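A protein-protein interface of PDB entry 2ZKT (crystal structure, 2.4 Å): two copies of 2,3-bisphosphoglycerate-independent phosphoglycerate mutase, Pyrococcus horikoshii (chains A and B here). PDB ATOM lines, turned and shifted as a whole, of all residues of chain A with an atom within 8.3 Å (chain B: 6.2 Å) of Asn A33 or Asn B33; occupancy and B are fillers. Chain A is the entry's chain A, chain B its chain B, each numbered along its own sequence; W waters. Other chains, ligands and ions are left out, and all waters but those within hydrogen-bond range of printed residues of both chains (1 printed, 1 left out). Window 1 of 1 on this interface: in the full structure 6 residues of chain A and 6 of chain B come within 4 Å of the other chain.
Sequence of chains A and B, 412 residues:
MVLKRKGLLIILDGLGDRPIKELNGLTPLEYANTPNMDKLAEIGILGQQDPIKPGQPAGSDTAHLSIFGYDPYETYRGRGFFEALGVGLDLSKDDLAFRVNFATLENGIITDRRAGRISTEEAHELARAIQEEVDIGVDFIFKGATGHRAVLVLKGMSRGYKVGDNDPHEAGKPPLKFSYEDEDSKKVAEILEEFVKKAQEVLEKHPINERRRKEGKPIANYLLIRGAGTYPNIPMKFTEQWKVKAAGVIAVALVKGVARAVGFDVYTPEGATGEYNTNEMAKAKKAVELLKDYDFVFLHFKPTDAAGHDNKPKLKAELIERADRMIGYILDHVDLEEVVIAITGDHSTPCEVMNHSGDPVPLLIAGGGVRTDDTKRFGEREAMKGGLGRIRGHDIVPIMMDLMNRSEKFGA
The backbone NH of Asn B33 lies within hydrogen-bond range of the side-chain carboxylate of Glu B321 (3.1 Å).
N of Asn A33 sits at hydrogen-bond distance from OE2 of Glu A321, at 2.9 Å.
Tyr A31 touches Pro B35.
Asn A33 touches Tyr B31 (OD1 to O, 3.96 Å).
Asn A33 touches Asn B33 (CG to CB, 3.8 Å).
Pro A35 touches Tyr B31 (CB to CE1, 3.9 Å).
Leu A26 touches none of the printed residues of chain B.
Of the printed residues of chain B, Tyr A31 touches Pro B35.
Asn A33 touches two residues of chain B.
Of the printed residues of chain B, Pro A35 touches Tyr B31 (3.9 Å).
Ala B32 touches none of the printed residues of chain A.
Printed residues of chain A within 4 Å of Asn B33: Asn A33 (3.8 Å).
Printed residues of chain A within 4 Å of Pro B35: Tyr A31.
Glu B321 touches none of the printed residues of chain A.
The nearest printed residue of chain A that does not touch Asn B33 is Tyr A31 (4.01 Å).
Hydrophobic or aromatic side chains of chain B within 4 Å of the printed part of chain A: Tyr B31 and Pro B35.
Among the printed residues, 4 pairs touch across the chains.
Among the printed residues, no Asp or Glu carboxylate lies within 4 Å of a Lys or Arg side-chain nitrogen of the other chain.
Tyr A31 touches Pro B35, and with the chains exchanged Pro A35 touches Tyr B31.
Asn A33 touches Tyr B31, but with the chains exchanged Tyr A31 does not touch Asn B33 (4.01 Å).
Asn A33 touches its own counterpart, Asn B33.
Positions printed for both chains: 28, 29, 30, 31, 32, 33, 34, 35, 38, 317, 320, 321 and 324.
Water W1 lies within hydrogen-bond range of NH2 of Arg A377 (3.1 Å) and OD1 of Asn B33 (3.4 Å).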
ATOM      1  N   LEU A  26     -26.672 -25.165  11.586  1.00  0.00           N
ATOM      2  CA  LEU A  26     -25.574 -24.426  10.965  1.00  0.00           C
ATOM      3  C   LEU A  26     -24.330 -25.305  10.812  1.00  0.00           C
ATOM      4  O   LEU A  26     -24.249 -26.402  11.365  1.00  0.00           O
ATOM      5  CB  LEU A  26     -25.205 -23.209  11.824  1.00  0.00           C
ATOM      6  CG  LEU A  26     -26.325 -22.205  12.147  1.00  0.00           C
ATOM      7  CD1 LEU A  26     -25.803 -21.184  13.148  1.00  0.00           C
ATOM      8  CD2 LEU A  26     -26.783 -21.512  10.868  1.00  0.00           C
ATOM      9  N   PRO A  28     -20.036 -25.684  11.206  1.00  0.00           N
ATOM     10  CA  PRO A  28     -19.108 -25.167  12.220  1.00  0.00           C
ATOM     11  C   PRO A  28     -18.619 -23.753  11.891  1.00  0.00           C
ATOM     12  O   PRO A  28     -18.480 -22.917  12.790  1.00  0.00           O
ATOM     13  CB  PRO A  28     -17.979 -26.205  12.210  1.00  0.00           C
ATOM     14  CG  PRO A  28     -18.699 -27.482  11.816  1.00  0.00           C
ATOM     15  CD  PRO A  28     -19.595 -27.003  10.701  1.00  0.00           C
ATOM     16  N   LEU A  29     -18.366 -23.483  10.609  1.00  0.00           N
ATOM     17  CA  LEU A  29     -17.897 -22.156  10.180  1.00  0.00           C
ATOM     18  C   LEU A  29     -18.962 -21.068  10.408  1.00  0.00           C
ATOM     19  O   LEU A  29     -18.637 -19.935  10.795  1.00  0.00           O
ATOM     20  CB  LEU A  29     -17.501 -22.169   8.685  1.00  0.00           C
ATOM     21  CG  LEU A  29     -17.248 -20.806   8.008  1.00  0.00           C
ATOM     22  CD1 LEU A  29     -16.095 -20.064   8.699  1.00  0.00           C
ATOM     23  CD2 LEU A  29     -16.907 -21.025   6.541  1.00  0.00           C
ATOM     24  N   GLU A  30     -20.229 -21.401  10.168  1.00  0.00           N
ATOM     25  CA  GLU A  30     -21.300 -20.414  10.354  1.00  0.00           C
ATOM     26  C   GLU A  30     -21.564 -20.176  11.843  1.00  0.00           C
ATOM     27  O   GLU A  30     -21.821 -19.056  12.257  1.00  0.00           O
ATOM     28  CB  GLU A  30     -22.598 -20.879   9.655  1.00  0.00           C
ATOM     29  CG  GLU A  30     -22.427 -21.150   8.162  1.00  0.00           C
ATOM     30  CD  GLU A  30     -23.604 -21.903   7.536  1.00  0.00           C
ATOM     31  OE1 GLU A  30     -24.127 -22.861   8.162  1.00  0.00           O
ATOM     32  OE2 GLU A  30     -23.998 -21.545   6.404  1.00  0.00           O
ATOM     33  N   TYR A  31     -21.476 -21.245  12.635  1.00  0.00           N
ATOM     34  CA  TYR A  31     -21.723 -21.190  14.080  1.00  0.00           C
ATOM     35  C   TYR A  31     -20.591 -20.476  14.824  1.00  0.00           C
ATOM     36  O   TYR A  31     -20.830 -19.752  15.786  1.00  0.00           O
ATOM     37  CB  TYR A  31     -21.883 -22.620  14.615  1.00  0.00           C
ATOM     38  CG  TYR A  31     -22.131 -22.723  16.105  1.00  0.00           C
ATOM     39  CD1 TYR A  31     -21.061 -22.834  17.005  1.00  0.00           C
ATOM     40  CD2 TYR A  31     -23.428 -22.718  16.619  1.00  0.00           C
ATOM     41  CE1 TYR A  31     -21.283 -22.938  18.382  1.00  0.00           C
ATOM     42  CE2 TYR A  31     -23.665 -22.826  17.998  1.00  0.00           C
ATOM     43  CZ  TYR A  31     -22.587 -22.935  18.873  1.00  0.00           C
ATOM     44  OH  TYR A  31     -22.817 -23.053  20.234  1.00  0.00           O
ATOM     45  N   ALA A  32     -19.358 -20.684  14.366  1.00  0.00           N
ATOM     46  CA  ALA A  32     -18.190 -20.077  14.989  1.00  0.00           C
ATOM     47  C   ALA A  32     -18.208 -18.548  14.923  1.00  0.00           C
ATOM     48  O   ALA A  32     -18.654 -17.964  13.935  1.00  0.00           O
ATOM     49  CB  ALA A  32     -16.915 -20.615  14.327  1.00  0.00           C
ATOM     50  N   ASN A  33     -17.709 -17.909  15.981  1.00  0.00           N
ATOM     51  CA  ASN A  33     -17.657 -16.451  16.038  1.00  0.00           C
ATOM     52  C   ASN A  33     -16.433 -15.987  15.233  1.00  0.00           C
ATOM     53  O   ASN A  33     -15.293 -16.056  15.706  1.00  0.00           O
ATOM     54  CB  ASN A  33     -17.556 -15.996  17.503  1.00  0.00           C
ATOM     55  CG  ASN A  33     -17.553 -14.483  17.650  1.00  0.00           C
ATOM     56  OD1 ASN A  33     -18.302 -13.775  16.961  1.00  0.00           O
ATOM     57  ND2 ASN A  33     -16.724 -13.978  18.560  1.00  0.00           N
ATOM     58  N   THR A  34     -16.681 -15.507  14.015  1.00  0.00           N
ATOM     59  CA  THR A  34     -15.598 -15.082  13.126  1.00  0.00           C
ATOM     60  C   THR A  34     -15.731 -13.637  12.613  1.00  0.00           C
ATOM     61  O   THR A  34     -15.943 -13.409  11.416  1.00  0.00           O
ATOM     62  CB  THR A  34     -15.521 -16.031  11.915  1.00  0.00           C
ATOM     63  OG1 THR A  34     -16.762 -15.971  11.186  1.00  0.00           O
ATOM     64  CG2 THR A  34     -15.321 -17.473  12.382  1.00  0.00           C
ATOM     65  N   PRO A  35     -15.597 -12.641  13.515  1.00  0.00           N
ATOM     66  CA  PRO A  35     -15.706 -11.226  13.117  1.00  0.00           C
ATOM     67  C   PRO A  35     -14.731 -10.789  12.011  1.00  0.00           C
ATOM     68  O   PRO A  35     -15.068  -9.961  11.160  1.00  0.00           O
ATOM     69  CB  PRO A  35     -15.475 -10.473  14.434  1.00  0.00           C
ATOM     70  CG  PRO A  35     -14.667 -11.486  15.286  1.00  0.00           C
ATOM     71  CD  PRO A  35     -15.370 -12.768  14.973  1.00  0.00           C
ATOM     72  N   ASN A  36     -13.531 -11.351  12.005  1.00  0.00           N
ATOM     73  CA  ASN A  36     -12.555 -10.961  10.991  1.00  0.00           C
ATOM     74  C   ASN A  36     -12.903 -11.489   9.583  1.00  0.00           C
ATOM     75  O   ASN A  36     -12.826 -10.747   8.592  1.00  0.00           O
ATOM     76  CB  ASN A  36     -11.145 -11.398  11.435  1.00  0.00           C
ATOM     77  CG  ASN A  36     -10.726 -10.740  12.763  1.00  0.00           C
ATOM     78  OD1 ASN A  36     -10.605  -9.517  12.854  1.00  0.00           O
ATOM     79  ND2 ASN A  36     -10.521 -11.558  13.798  1.00  0.00           N
ATOM     80  N   MET A  37     -13.297 -12.756   9.481  1.00  0.00           N
ATOM     81  CA  MET A  37     -13.665 -13.282   8.171  1.00  0.00           C
ATOM     82  C   MET A  37     -14.991 -12.640   7.725  1.00  0.00           C
ATOM     83  O   MET A  37     -15.143 -12.285   6.559  1.00  0.00           O
ATOM     84  CB  MET A  37     -13.748 -14.821   8.202  1.00  0.00           C
ATOM     85  CG  MET A  37     -12.356 -15.478   8.320  1.00  0.00           C
ATOM     86  SD  MET A  37     -12.279 -17.293   8.101  1.00  0.00           S
ATOM     87  CE  MET A  37     -12.452 -17.861   9.800  1.00  0.00           C
ATOM     88  N   ASP A  38     -15.937 -12.457   8.651  1.00  0.00           N
ATOM     89  CA  ASP A  38     -17.217 -11.824   8.288  1.00  0.00           C
ATOM     90  C   ASP A  38     -16.946 -10.414   7.743  1.00  0.00           C
ATOM     91  O   ASP A  38     -17.533  -9.984   6.730  1.00  0.00           O
ATOM     92  CB  ASP A  38     -18.161 -11.738   9.503  1.00  0.00           C
ATOM     93  CG  ASP A  38     -18.637 -13.121   9.998  1.00  0.00           C
ATOM     94  OD1 ASP A  38     -18.364 -14.143   9.317  1.00  0.00           O
ATOM     95  OD2 ASP A  38     -19.296 -13.172  11.076  1.00  0.00           O
ATOM     96  N   ALA A 317     -15.357 -25.675  15.295  1.00  0.00           N
ATOM     97  CA  ALA A 317     -15.751 -24.271  15.423  1.00  0.00           C
ATOM     98  C   ALA A 317     -14.697 -23.482  16.204  1.00  0.00           C
ATOM     99  O   ALA A 317     -14.297 -22.381  15.795  1.00  0.00           O
ATOM    100  CB  ALA A 317     -17.114 -24.159  16.122  1.00  0.00           C
ATOM    101  N   GLU A 318     -14.245 -24.050  17.328  1.00  0.00           N
ATOM    102  CA  GLU A 318     -13.239 -23.383  18.161  1.00  0.00           C
ATOM    103  C   GLU A 318     -11.966 -23.162  17.342  1.00  0.00           C
ATOM    104  O   GLU A 318     -11.379 -22.068  17.361  1.00  0.00           O
ATOM    105  CB  GLU A 318     -12.927 -24.228  19.400  1.00  0.00           C
ATOM    106  CG  GLU A 318     -12.022 -23.522  20.401  1.00  0.00           C
ATOM    107  CD  GLU A 318     -11.792 -24.335  21.663  1.00  0.00           C
ATOM    108  OE1 GLU A 318     -11.207 -25.445  21.566  1.00  0.00           O
ATOM    109  OE2 GLU A 318     -12.198 -23.863  22.755  1.00  0.00           O
ATOM    110  N   ILE A 320     -11.750 -22.930  14.139  1.00  0.00           N
ATOM    111  CA  ILE A 320     -12.047 -21.896  13.149  1.00  0.00           C
ATOM    112  C   ILE A 320     -11.956 -20.516  13.808  1.00  0.00           C
ATOM    113  O   ILE A 320     -11.485 -19.554  13.197  1.00  0.00           O
ATOM    114  CB  ILE A 320     -13.453 -22.102  12.515  1.00  0.00           C
ATOM    115  CG1 ILE A 320     -13.397 -23.294  11.540  1.00  0.00           C
ATOM    116  CG2 ILE A 320     -13.900 -20.829  11.784  1.00  0.00           C
ATOM    117  CD1 ILE A 320     -14.728 -23.954  11.279  1.00  0.00           C
ATOM    118  N   GLU A 321     -12.386 -20.424  15.069  1.00  0.00           N
ATOM    119  CA  GLU A 321     -12.317 -19.149  15.787  1.00  0.00           C
ATOM    120  C   GLU A 321     -10.845 -18.747  15.973  1.00  0.00           C
ATOM    121  O   GLU A 321     -10.482 -17.572  15.834  1.00  0.00           O
ATOM    122  CB  GLU A 321     -13.041 -19.266  17.139  1.00  0.00           C
ATOM    123  CG  GLU A 321     -14.506 -19.693  16.987  1.00  0.00           C
ATOM    124  CD  GLU A 321     -15.294 -19.661  18.294  1.00  0.00           C
ATOM    125  OE1 GLU A 321     -14.821 -20.247  19.297  1.00  0.00           O
ATOM    126  OE2 GLU A 321     -16.394 -19.057  18.313  1.00  0.00           O
ATOM    127  N   ARG A 322      -9.993 -19.728  16.270  1.00  0.00           N
ATOM    128  CA  ARG A 322      -8.564 -19.455  16.448  1.00  0.00           C
ATOM    129  C   ARG A 322      -7.984 -18.928  15.133  1.00  0.00           C
ATOM    130  O   ARG A 322      -7.116 -18.048  15.124  1.00  0.00           O
ATOM    131  CB  ARG A 322      -7.825 -20.732  16.904  1.00  0.00           C
ATOM    132  CG  ARG A 322      -8.049 -21.062  18.392  1.00  0.00           C
ATOM    133  CD  ARG A 322      -7.563 -22.453  18.767  1.00  0.00           C
ATOM    134  NE  ARG A 322      -6.148 -22.651  18.448  1.00  0.00           N
ATOM    135  CZ  ARG A 322      -5.494 -23.799  18.638  1.00  0.00           C
ATOM    136  NH1 ARG A 322      -6.129 -24.852  19.159  1.00  0.00           N
ATOM    137  NH2 ARG A 322      -4.220 -23.908  18.266  1.00  0.00           N
ATOM    138  N   ALA A 323      -8.486 -19.456  14.017  1.00  0.00           N
ATOM    139  CA  ALA A 323      -8.016 -19.020  12.709  1.00  0.00           C
ATOM    140  C   ALA A 323      -8.437 -17.566  12.497  1.00  0.00           C
ATOM    141  O   ALA A 323      -7.680 -16.766  11.928  1.00  0.00           O
ATOM    142  CB  ALA A 323      -8.603 -19.916  11.618  1.00  0.00           C
ATOM    143  N   ASP A 324      -9.642 -17.221  12.968  1.00  0.00           N
ATOM    144  CA  ASP A 324     -10.147 -15.855  12.809  1.00  0.00           C
ATOM    145  C   ASP A 324      -9.256 -14.867  13.558  1.00  0.00           C
ATOM    146  O   ASP A 324      -9.026 -13.745  13.082  1.00  0.00           O
ATOM    147  CB  ASP A 324     -11.598 -15.725  13.315  1.00  0.00           C
ATOM    148  CG  ASP A 324     -12.267 -14.419  12.852  1.00  0.00           C
ATOM    149  OD1 ASP A 324     -12.470 -14.251  11.625  1.00  0.00           O
ATOM    150  OD2 ASP A 324     -12.584 -13.554  13.705  1.00  0.00           O
ATOM    151  N   ARG A 325      -8.762 -15.270  14.733  1.00  0.00           N
ATOM    152  CA  ARG A 325      -7.881 -14.391  15.509  1.00  0.00           C
ATOM    153  C   ARG A 325      -6.600 -14.221  14.701  1.00  0.00           C
ATOM    154  O   ARG A 325      -6.137 -13.098  14.468  1.00  0.00           O
ATOM    155  CB  ARG A 325      -7.572 -14.998  16.888  1.00  0.00           C
ATOM    156  CG  ARG A 325      -8.664 -14.741  17.932  1.00  0.00           C
ATOM    157  CD  ARG A 325      -8.222 -15.152  19.346  1.00  0.00           C
ATOM    158  NE  ARG A 325      -8.588 -16.532  19.682  1.00  0.00           N
ATOM    159  CZ  ARG A 325      -9.841 -16.945  19.879  1.00  0.00           C
ATOM    160  NH1 ARG A 325     -10.851 -16.082  19.774  1.00  0.00           N
ATOM    161  NH2 ARG A 325     -10.086 -18.217  20.189  1.00  0.00           N
ATOM    162  N   ARG A 377     -21.401 -12.193   5.729  1.00  0.00           N
ATOM    163  CA  ARG A 377     -20.695 -13.138   6.594  1.00  0.00           C
ATOM    164  C   ARG A 377     -20.003 -14.204   5.757  1.00  0.00           C
ATOM    165  O   ARG A 377     -20.269 -14.335   4.556  1.00  0.00           O
ATOM    166  CB  ARG A 377     -21.677 -13.838   7.549  1.00  0.00           C
ATOM    167  CG  ARG A 377     -22.126 -13.018   8.747  1.00  0.00           C
ATOM    168  CD  ARG A 377     -22.862 -13.911   9.748  1.00  0.00           C
ATOM    169  NE  ARG A 377     -22.839 -13.352  11.102  1.00  0.00           N
ATOM    170  CZ  ARG A 377     -23.151 -14.032  12.208  1.00  0.00           C
ATOM    171  NH1 ARG A 377     -23.514 -15.311  12.132  1.00  0.00           N
ATOM    172  NH2 ARG A 377     -23.097 -13.431  13.398  1.00  0.00           N
ATOM    173  N   PRO B  28     -23.100  -3.709  19.335  1.00  0.00           N
ATOM    174  CA  PRO B  28     -22.679  -4.746  20.290  1.00  0.00           C
ATOM    175  C   PRO B  28     -23.512  -6.026  20.141  1.00  0.00           C
ATOM    176  O   PRO B  28     -22.983  -7.134  20.228  1.00  0.00           O
ATOM    177  CB  PRO B  28     -22.897  -4.065  21.647  1.00  0.00           C
ATOM    178  CG  PRO B  28     -22.520  -2.639  21.337  1.00  0.00           C
ATOM    179  CD  PRO B  28     -23.214  -2.394  20.002  1.00  0.00           C
ATOM    180  N   LEU B  29     -24.814  -5.864  19.914  1.00  0.00           N
ATOM    181  CA  LEU B  29     -25.708  -7.007  19.763  1.00  0.00           C
ATOM    182  C   LEU B  29     -25.393  -7.822  18.518  1.00  0.00           C
ATOM    183  O   LEU B  29     -25.461  -9.048  18.548  1.00  0.00           O
ATOM    184  CB  LEU B  29     -27.180  -6.554  19.697  1.00  0.00           C
ATOM    185  CG  LEU B  29     -28.180  -7.662  19.274  1.00  0.00           C
ATOM    186  CD1 LEU B  29     -28.015  -8.907  20.148  1.00  0.00           C
ATOM    187  CD2 LEU B  29     -29.605  -7.117  19.381  1.00  0.00           C
ATOM    188  N   GLU B  30     -25.042  -7.143  17.428  1.00  0.00           N
ATOM    189  CA  GLU B  30     -24.736  -7.843  16.186  1.00  0.00           C
ATOM    190  C   GLU B  30     -23.379  -8.541  16.304  1.00  0.00           C
ATOM    191  O   GLU B  30     -23.250  -9.733  15.996  1.00  0.00           O
ATOM    192  CB  GLU B  30     -24.752  -6.854  15.003  1.00  0.00           C
ATOM    193  CG  GLU B  30     -26.140  -6.277  14.723  1.00  0.00           C
ATOM    194  CD  GLU B  30     -26.112  -5.044  13.819  1.00  0.00           C
ATOM    195  OE1 GLU B  30     -25.103  -4.293  13.857  1.00  0.00           O
ATOM    196  OE2 GLU B  30     -27.112  -4.813  13.082  1.00  0.00           O
ATOM    197  N   TYR B  31     -22.391  -7.782  16.790  1.00  0.00           N
ATOM    198  CA  TYR B  31     -21.010  -8.244  16.987  1.00  0.00           C
ATOM    199  C   TYR B  31     -20.938  -9.427  17.970  1.00  0.00           C
ATOM    200  O   TYR B  31     -20.269 -10.415  17.708  1.00  0.00           O
ATOM    201  CB  TYR B  31     -20.164  -7.074  17.524  1.00  0.00           C
ATOM    202  CG  TYR B  31     -18.703  -7.391  17.784  1.00  0.00           C
ATOM    203  CD1 TYR B  31     -17.774  -7.412  16.739  1.00  0.00           C
ATOM    204  CD2 TYR B  31     -18.242  -7.652  19.080  1.00  0.00           C
ATOM    205  CE1 TYR B  31     -16.427  -7.684  16.974  1.00  0.00           C
ATOM    206  CE2 TYR B  31     -16.889  -7.926  19.327  1.00  0.00           C
ATOM    207  CZ  TYR B  31     -15.989  -7.939  18.268  1.00  0.00           C
ATOM    208  OH  TYR B  31     -14.647  -8.206  18.495  1.00  0.00           O
ATOM    209  N   ALA B  32     -21.636  -9.306  19.102  1.00  0.00           N
ATOM    210  CA  ALA B  32     -21.648 -10.343  20.135  1.00  0.00           C
ATOM    211  C   ALA B  32     -22.083 -11.693  19.589  1.00  0.00           C
ATOM    212  O   ALA B  32     -22.987 -11.774  18.773  1.00  0.00           O
ATOM    213  CB  ALA B  32     -22.581  -9.923  21.282  1.00  0.00           C
ATOM    214  N   ASN B  33     -21.433 -12.760  20.046  1.00  0.00           N
ATOM    215  CA  ASN B  33     -21.783 -14.109  19.611  1.00  0.00           C
ATOM    216  C   ASN B  33     -23.022 -14.530  20.411  1.00  0.00           C
ATOM    217  O   ASN B  33     -22.940 -14.803  21.613  1.00  0.00           O
ATOM    218  CB  ASN B  33     -20.604 -15.060  19.879  1.00  0.00           C
ATOM    219  CG  ASN B  33     -20.899 -16.496  19.473  1.00  0.00           C
ATOM    220  OD1 ASN B  33     -21.407 -16.751  18.382  1.00  0.00           O
ATOM    221  ND2 ASN B  33     -20.566 -17.440  20.349  1.00  0.00           N
ATOM    222  N   THR B  34     -24.169 -14.584  19.731  1.00  0.00           N
ATOM    223  CA  THR B  34     -25.444 -14.931  20.367  1.00  0.00           C
ATOM    224  C   THR B  34     -26.197 -16.008  19.583  1.00  0.00           C
ATOM    225  O   THR B  34     -27.294 -15.762  19.064  1.00  0.00           O
ATOM    226  CB  THR B  34     -26.351 -13.684  20.458  1.00  0.00           C
ATOM    227  OG1 THR B  34     -26.638 -13.213  19.126  1.00  0.00           O
ATOM    228  CG2 THR B  34     -25.647 -12.560  21.223  1.00  0.00           C
ATOM    229  N   PRO B  35     -25.640 -17.232  19.524  1.00  0.00           N
ATOM    230  CA  PRO B  35     -26.291 -18.323  18.781  1.00  0.00           C
ATOM    231  C   PRO B  35     -27.731 -18.665  19.180  1.00  0.00           C
ATOM    232  O   PRO B  35     -28.504 -19.125  18.342  1.00  0.00           O
ATOM    233  CB  PRO B  35     -25.329 -19.495  18.988  1.00  0.00           C
ATOM    234  CG  PRO B  35     -24.791 -19.245  20.371  1.00  0.00           C
ATOM    235  CD  PRO B  35     -24.507 -17.747  20.330  1.00  0.00           C
ATOM    236  N   ASP B  38     -30.157 -15.905  17.869  1.00  0.00           N
ATOM    237  CA  ASP B  38     -30.176 -16.057  16.404  1.00  0.00           C
ATOM    238  C   ASP B  38     -31.076 -17.245  16.024  1.00  0.00           C
ATOM    239  O   ASP B  38     -31.782 -17.205  15.012  1.00  0.00           O
ATOM    240  CB  ASP B  38     -28.765 -16.313  15.836  1.00  0.00           C
ATOM    241  CG  ASP B  38     -27.832 -15.104  15.986  1.00  0.00           C
ATOM    242  OD1 ASP B  38     -28.275 -14.072  16.556  1.00  0.00           O
ATOM    243  OD2 ASP B  38     -26.656 -15.194  15.536  1.00  0.00           O
ATOM    244  N   ALA B 317     -21.069  -5.977  24.561  1.00  0.00           N
ATOM    245  CA  ALA B 317     -21.216  -7.156  23.708  1.00  0.00           C
ATOM    246  C   ALA B 317     -20.949  -8.412  24.556  1.00  0.00           C
ATOM    247  O   ALA B 317     -21.654  -9.421  24.434  1.00  0.00           O
ATOM    248  CB  ALA B 317     -20.230  -7.088  22.522  1.00  0.00           C
ATOM    249  N   ILE B 320     -23.992  -9.030  26.558  1.00  0.00           N
ATOM    250  CA  ILE B 320     -25.090  -9.587  25.767  1.00  0.00           C
ATOM    251  C   ILE B 320     -24.877 -11.087  25.542  1.00  0.00           C
ATOM    252  O   ILE B 320     -25.815 -11.865  25.387  1.00  0.00           O
ATOM    253  CB  ILE B 320     -25.214  -8.841  24.414  1.00  0.00           C
ATOM    254  CG1 ILE B 320     -25.682  -7.387  24.636  1.00  0.00           C
ATOM    255  CG2 ILE B 320     -26.270  -9.538  23.527  1.00  0.00           C
ATOM    256  CD1 ILE B 320     -25.687  -6.546  23.343  1.00  0.00           C
ATOM    257  N   GLU B 321     -23.580 -11.480  25.511  1.00  0.00           N
ATOM    258  CA  GLU B 321     -23.259 -12.901  25.351  1.00  0.00           C
ATOM    259  C   GLU B 321     -23.625 -13.707  26.605  1.00  0.00           C
ATOM    260  O   GLU B 321     -24.051 -14.851  26.527  1.00  0.00           O
ATOM    261  CB  GLU B 321     -21.757 -13.053  25.031  1.00  0.00           C
ATOM    262  CG  GLU B 321     -21.443 -12.874  23.534  1.00  0.00           C
ATOM    263  CD  GLU B 321     -19.960 -13.081  23.261  1.00  0.00           C
ATOM    264  OE1 GLU B 321     -19.362 -13.962  23.861  1.00  0.00           O
ATOM    265  OE2 GLU B 321     -19.422 -12.384  22.407  1.00  0.00           O
ATOM    266  N   ASP B 324     -27.153 -14.359  26.306  1.00  0.00           N
ATOM    267  CA  ASP B 324     -27.479 -15.422  25.355  1.00  0.00           C
ATOM    268  C   ASP B 324     -27.394 -16.792  26.020  1.00  0.00           C
ATOM    269  O   ASP B 324     -28.261 -17.653  25.800  1.00  0.00           O
ATOM    270  CB  ASP B 324     -26.561 -15.385  24.121  1.00  0.00           C
ATOM    271  CG  ASP B 324     -27.157 -16.144  22.928  1.00  0.00           C
ATOM    272  OD1 ASP B 324     -28.252 -15.745  22.458  1.00  0.00           O
ATOM    273  OD2 ASP B 324     -26.543 -17.139  22.457  1.00  0.00           O
HETATM  274  O   HOH W   1     -21.568 -14.835  15.633  1.00  0.00           O
